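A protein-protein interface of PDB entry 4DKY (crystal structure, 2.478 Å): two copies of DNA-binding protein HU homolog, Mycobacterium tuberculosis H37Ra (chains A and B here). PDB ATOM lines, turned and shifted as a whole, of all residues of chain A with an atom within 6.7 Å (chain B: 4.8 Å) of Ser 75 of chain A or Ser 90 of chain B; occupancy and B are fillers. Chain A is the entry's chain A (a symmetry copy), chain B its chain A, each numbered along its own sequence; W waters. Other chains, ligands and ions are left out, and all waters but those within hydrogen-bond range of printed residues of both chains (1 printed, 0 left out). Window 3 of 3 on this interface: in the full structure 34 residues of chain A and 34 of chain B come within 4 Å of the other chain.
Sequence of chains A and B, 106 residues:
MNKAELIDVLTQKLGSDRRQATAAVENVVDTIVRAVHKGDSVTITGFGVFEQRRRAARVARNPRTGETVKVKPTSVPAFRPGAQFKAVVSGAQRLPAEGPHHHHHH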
ATOM      1  N   HIS A  37     -26.936 -23.738  -1.424  1.00  0.00           N
ATOM      2  CA  HIS A  37     -25.892 -22.799  -1.859  1.00  0.00           C
ATOM      3  C   HIS A  37     -26.531 -21.500  -2.249  1.00  0.00           C
ATOM      4  O   HIS A  37     -26.082 -20.491  -1.877  1.00  0.00           O
ATOM      5  CB  HIS A  37     -25.110 -23.418  -3.011  1.00  0.00           C
ATOM      6  CG  HIS A  37     -24.374 -22.408  -3.809  1.00  0.00           C
ATOM      7  ND1 HIS A  37     -24.805 -21.956  -5.001  1.00  0.00           N
ATOM      8  CD2 HIS A  37     -23.217 -21.721  -3.540  1.00  0.00           C
ATOM      9  CE1 HIS A  37     -23.934 -21.057  -5.489  1.00  0.00           C
ATOM     10  NE2 HIS A  37     -22.971 -20.894  -4.604  1.00  0.00           N
ATOM     11  N   GLN A  52     -29.336 -23.075   4.657  1.00  0.00           N
ATOM     12  CA  GLN A  52     -28.157 -22.233   4.806  1.00  0.00           C
ATOM     13  C   GLN A  52     -28.362 -21.391   6.135  1.00  0.00           C
ATOM     14  O   GLN A  52     -29.481 -20.936   6.416  1.00  0.00           O
ATOM     15  CB  GLN A  52     -28.039 -21.348   3.558  1.00  0.00           C
ATOM     16  CG  GLN A  52     -27.341 -20.061   3.740  1.00  0.00           C
ATOM     17  CD  GLN A  52     -26.867 -19.445   2.432  1.00  0.00           C
ATOM     18  OE1 GLN A  52     -26.533 -20.129   1.440  1.00  0.00           O
ATOM     19  NE2 GLN A  52     -26.834 -18.118   2.410  1.00  0.00           N
ATOM     20  N   ARG A  53     -27.301 -21.220   6.931  1.00  0.00           N
ATOM     21  CA  ARG A  53     -27.360 -20.357   8.105  1.00  0.00           C
ATOM     22  C   ARG A  53     -26.138 -19.461   8.049  1.00  0.00           C
ATOM     23  O   ARG A  53     -25.119 -19.805   7.442  1.00  0.00           O
ATOM     24  CB  ARG A  53     -27.338 -21.166   9.387  1.00  0.00           C
ATOM     25  CG  ARG A  53     -28.705 -21.785   9.721  1.00  0.00           C
ATOM     26  CD  ARG A  53     -28.493 -22.703  10.911  1.00  0.00           C
ATOM     27  NE  ARG A  53     -29.586 -23.604  11.152  1.00  0.00           N
ATOM     28  CZ  ARG A  53     -29.508 -24.634  12.005  1.00  0.00           C
ATOM     29  NH1 ARG A  53     -28.424 -24.828  12.723  1.00  0.00           N
ATOM     30  NH2 ARG A  53     -30.546 -25.486  12.163  1.00  0.00           N
ATOM     31  N   ARG A  54     -26.287 -18.322   8.672  1.00  0.00           N
ATOM     32  CA  ARG A  54     -25.291 -17.316   8.684  1.00  0.00           C
ATOM     33  C   ARG A  54     -24.684 -17.190  10.038  1.00  0.00           C
ATOM     34  O   ARG A  54     -25.308 -16.854  10.980  1.00  0.00           O
ATOM     35  CB  ARG A  54     -25.918 -16.002   8.288  1.00  0.00           C
ATOM     36  CG  ARG A  54     -24.962 -14.847   8.273  1.00  0.00           C
ATOM     37  CD  ARG A  54     -24.489 -14.524   6.869  1.00  0.00           C
ATOM     38  NE  ARG A  54     -23.887 -13.207   6.847  1.00  0.00           N
ATOM     39  CZ  ARG A  54     -23.896 -12.370   7.887  1.00  0.00           C
ATOM     40  NH1 ARG A  54     -24.473 -12.723   9.024  1.00  0.00           N
ATOM     41  NH2 ARG A  54     -23.332 -11.177   7.794  1.00  0.00           N
ATOM     42  N   ARG A  55     -23.421 -17.465  10.090  1.00  0.00           N
ATOM     43  CA  ARG A  55     -22.620 -17.138  11.258  1.00  0.00           C
ATOM     44  C   ARG A  55     -22.080 -15.686  11.326  1.00  0.00           C
ATOM     45  O   ARG A  55     -21.305 -15.258  10.461  1.00  0.00           O
ATOM     46  CB  ARG A  55     -21.491 -18.096  11.380  1.00  0.00           C
ATOM     47  CG  ARG A  55     -21.988 -19.333  11.940  1.00  0.00           C
ATOM     48  CD  ARG A  55     -20.803 -20.147  12.274  1.00  0.00           C
ATOM     49  NE  ARG A  55     -21.289 -21.511  12.368  1.00  0.00           N
ATOM     50  CZ  ARG A  55     -20.515 -22.579  12.202  1.00  0.00           C
ATOM     51  NH1 ARG A  55     -19.190 -22.436  11.914  1.00  0.00           N
ATOM     52  NH2 ARG A  55     -21.052 -23.800  12.289  1.00  0.00           N
ATOM     53  N   PRO A  73     -17.974 -12.976   9.154  1.00  0.00           N
ATOM     54  CA  PRO A  73     -19.233 -13.750   8.993  1.00  0.00           C
ATOM     55  C   PRO A  73     -19.192 -14.753   7.815  1.00  0.00           C
ATOM     56  O   PRO A  73     -18.574 -14.475   6.777  1.00  0.00           O
ATOM     57  CB  PRO A  73     -20.331 -12.680   8.760  1.00  0.00           C
ATOM     58  CG  PRO A  73     -19.722 -11.420   9.056  1.00  0.00           C
ATOM     59  CD  PRO A  73     -18.188 -11.545   8.993  1.00  0.00           C
ATOM     60  N   THR A  74     -19.868 -15.878   7.984  1.00  0.00           N
ATOM     61  CA  THR A  74     -19.786 -16.971   7.048  1.00  0.00           C
ATOM     62  C   THR A  74     -21.122 -17.621   6.876  1.00  0.00           C
ATOM     63  O   THR A  74     -21.900 -17.664   7.794  1.00  0.00           O
ATOM     64  CB  THR A  74     -18.811 -18.003   7.639  1.00  0.00           C
ATOM     65  OG1 THR A  74     -17.520 -17.396   7.730  1.00  0.00           O
ATOM     66  CG2 THR A  74     -18.716 -19.304   6.783  1.00  0.00           C
ATOM     67  N   SER A  75     -21.407 -18.131   5.710  1.00  0.00           N
ATOM     68  CA  SER A  75     -22.642 -18.889   5.502  1.00  0.00           C
ATOM     69  C   SER A  75     -22.344 -20.330   5.666  1.00  0.00           C
ATOM     70  O   SER A  75     -21.320 -20.820   5.169  1.00  0.00           O
ATOM     71  CB  SER A  75     -23.139 -18.698   4.113  1.00  0.00           C
ATOM     72  OG  SER A  75     -23.719 -17.386   3.972  1.00  0.00           O
ATOM     73  N   VAL A  76     -23.197 -21.043   6.405  1.00  0.00           N
ATOM     74  CA  VAL A  76     -22.921 -22.510   6.581  1.00  0.00           C
ATOM     75  C   VAL A  76     -24.136 -23.381   6.220  1.00  0.00           C
ATOM     76  O   VAL A  76     -25.274 -22.932   6.272  1.00  0.00           O
ATOM     77  CB  VAL A  76     -22.506 -22.834   7.982  1.00  0.00           C
ATOM     78  CG1 VAL A  76     -21.128 -22.121   8.398  1.00  0.00           C
ATOM     79  CG2 VAL A  76     -23.628 -22.435   8.894  1.00  0.00           C
ATOM     80  N   PRO A  77     -23.906 -24.626   5.913  1.00  0.00           N
ATOM     81  CA  PRO A  77     -25.059 -25.494   5.680  1.00  0.00           C
ATOM     82  C   PRO A  77     -25.561 -26.132   6.983  1.00  0.00           C
ATOM     83  O   PRO A  77     -24.793 -26.367   7.899  1.00  0.00           O
ATOM     84  CB  PRO A  77     -24.456 -26.559   4.699  1.00  0.00           C
ATOM     85  CG  PRO A  77     -23.020 -26.532   4.968  1.00  0.00           C
ATOM     86  CD  PRO A  77     -22.655 -25.267   5.608  1.00  0.00           C
ATOM     87  N   LYS B  86     -19.631 -27.673   3.003  1.00  0.00           N
ATOM     88  CA  LYS B  86     -19.238 -26.380   3.720  1.00  0.00           C
ATOM     89  C   LYS B  86     -18.523 -25.362   2.797  1.00  0.00           C
ATOM     90  O   LYS B  86     -18.920 -24.202   2.710  1.00  0.00           O
ATOM     91  CB  LYS B  86     -18.313 -26.653   4.899  1.00  0.00           C
ATOM     92  CG  LYS B  86     -19.024 -27.230   6.064  1.00  0.00           C
ATOM     93  CD  LYS B  86     -18.052 -27.271   7.208  1.00  0.00           C
ATOM     94  CE  LYS B  86     -17.530 -28.717   7.315  1.00  0.00           C
ATOM     95  NZ  LYS B  86     -16.628 -29.005   8.515  1.00  0.00           N
ATOM     96  N   ALA B  87     -17.535 -25.883   2.095  1.00  0.00           N
ATOM     97  CA  ALA B  87     -16.700 -25.107   1.092  1.00  0.00           C
ATOM     98  C   ALA B  87     -17.469 -24.331   0.037  1.00  0.00           C
ATOM     99  O   ALA B  87     -17.189 -23.183  -0.279  1.00  0.00           O
ATOM    100  CB  ALA B  87     -15.707 -25.996   0.446  1.00  0.00           C
ATOM    101  N   VAL B  88     -18.459 -25.015  -0.493  1.00  0.00           N
ATOM    102  CA  VAL B  88     -19.381 -24.461  -1.454  1.00  0.00           C
ATOM    103  C   VAL B  88     -20.339 -23.477  -0.872  1.00  0.00           C
ATOM    104  O   VAL B  88     -20.555 -22.411  -1.435  1.00  0.00           O
ATOM    105  CB  VAL B  88     -20.157 -25.609  -2.117  1.00  0.00           C
ATOM    106  CG1 VAL B  88     -21.500 -25.124  -2.646  1.00  0.00           C
ATOM    107  CG2 VAL B  88     -19.346 -26.219  -3.266  1.00  0.00           C
ATOM    108  N   VAL B  89     -20.957 -23.820   0.259  1.00  0.00           N
ATOM    109  CA  VAL B  89     -21.906 -22.872   0.915  1.00  0.00           C
ATOM    110  C   VAL B  89     -21.202 -21.587   1.290  1.00  0.00           C
ATOM    111  O   VAL B  89     -21.667 -20.449   0.952  1.00  0.00           O
ATOM    112  CB  VAL B  89     -22.565 -23.506   2.120  1.00  0.00           C
ATOM    113  CG1 VAL B  89     -23.546 -22.602   2.844  1.00  0.00           C
ATOM    114  CG2 VAL B  89     -23.278 -24.644   1.584  1.00  0.00           C
ATOM    115  N   SER B  90     -20.057 -21.775   1.944  1.00  0.00           N
ATOM    116  CA  SER B  90     -19.233 -20.601   2.386  1.00  0.00           C
ATOM    117  C   SER B  90     -18.739 -19.706   1.286  1.00  0.00           C
ATOM    118  O   SER B  90     -18.531 -18.553   1.532  1.00  0.00           O
ATOM    119  CB  SER B  90     -17.971 -21.026   3.113  1.00  0.00           C
ATOM    120  OG  SER B  90     -16.961 -21.312   2.152  1.00  0.00           O
ATOM    121  N   GLY B  91     -18.500 -20.245   0.103  1.00  0.00           N
ATOM    122  CA  GLY B  91     -18.020 -19.444  -1.007  1.00  0.00           C
ATOM    123  C   GLY B  91     -16.598 -19.844  -1.329  1.00  0.00           C
ATOM    124  O   GLY B  91     -16.031 -19.374  -2.281  1.00  0.00           O
ATOM    125  N   ALA B  92     -16.022 -20.741  -0.559  1.00  0.00           N
ATOM    126  CA  ALA B  92     -14.605 -21.098  -0.799  1.00  0.00           C
ATOM    127  C   ALA B  92     -14.331 -21.879  -2.130  1.00  0.00           C
ATOM    128  O   ALA B  92     -13.385 -21.612  -2.851  1.00  0.00           O
ATOM    129  CB  ALA B  92     -14.000 -21.818   0.404  1.00  0.00           C
HETATM  130  O   HOH W   1     -19.844 -17.118   3.388  1.00  0.00           O
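The side-chain amide oxygen of Gln 52 of chain A sits close to the backbone carbonyl oxygen of His 37 of chain A. OG of Ser 90 of chain B is in hydrogen-bond range of O of Ala 87 of chain B. The backbone NH (N) of Val 76 of chain A is in hydrogen-bond range of the backbone carbonyl oxygen (O) of Arg 53 of chain A. The side-chain hydroxyl of Ser 90 of chain B is in hydrogen-bond range of the backbone NH of Ala 92 of chain B (2.9 Å).
His 37 of chain A touches Val 88 of chain B (CD2 to O, 3.5 Å). CG1 of Val 89 of chain B touches O of Ser 75 of chain A (3.7 Å). O of Ser 75 of chain A touches CA of Ser 90 of chain B, at 3.5 Å. Val 89 of chain B touches Val 76 of chain A (CG1 to C, 3.5 Å). CA of Lys 86 of chain B touches CG of Pro 77 of chain A (3.99 Å). N of Pro 77 of chain A touches CG1 of Val 89 of chain B (3.7 Å).
Of chain B, only Val 89 (3.7 Å) and Ser 90 (3.5 Å) come within 4 Å of Ser 75 of chain A. Of the printed residues of chain A, Ser 90 of chain B touches Ser 75 (3.5 Å). Printed residues of chain B within 4 Å of Val 76 of chain A: Val 89 (3.5 Å). Printed residues of chain B within 4 Å of His 37 of chain A: Val 88. Printed residues of chain A within 4 Å of Lys 86 of chain B: Pro 77 (3.99 Å). The nearest printed residue of chain B that does not touch Ser 75 of chain A is Lys 86 of chain B (4.8 Å). The nearest printed residue of chain A that does not touch Lys 86 of chain B is Ser 75 of chain A (4.8 Å).
Of the 10 printed residues of chain A, 4 touch a printed residue of chain B. Printed residues of chain A that touch a printed residue of chain B: His 37, Ser 75, Val 76 and Pro 77. Hydrophobic or aromatic side chains of chain A that line the printed part of chain B: His 37 and Pro 77. Along chain A the printed residues that touch a printed residue of chain B span positions 37 to 77. Printed residues of chain B that touch a printed residue of chain A: Lys 86, Val 88, Val 89 and Ser 90. Hydrophobic or aromatic side chains of chain B that line the printed part of chain A: Val 88 and Val 89. Among the printed residues, 6 pairs touch across the chains. Among the printed residues, no Asp or Glu carboxylate lies within 4 Å of a Lys or Arg side-chain nitrogen of the other chain.
No position is printed for both chains.
Water W1 bridges the backbone carbonyl oxygen of Ser 90 of chain B and the backbone NH of Ser 75 of chain A.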
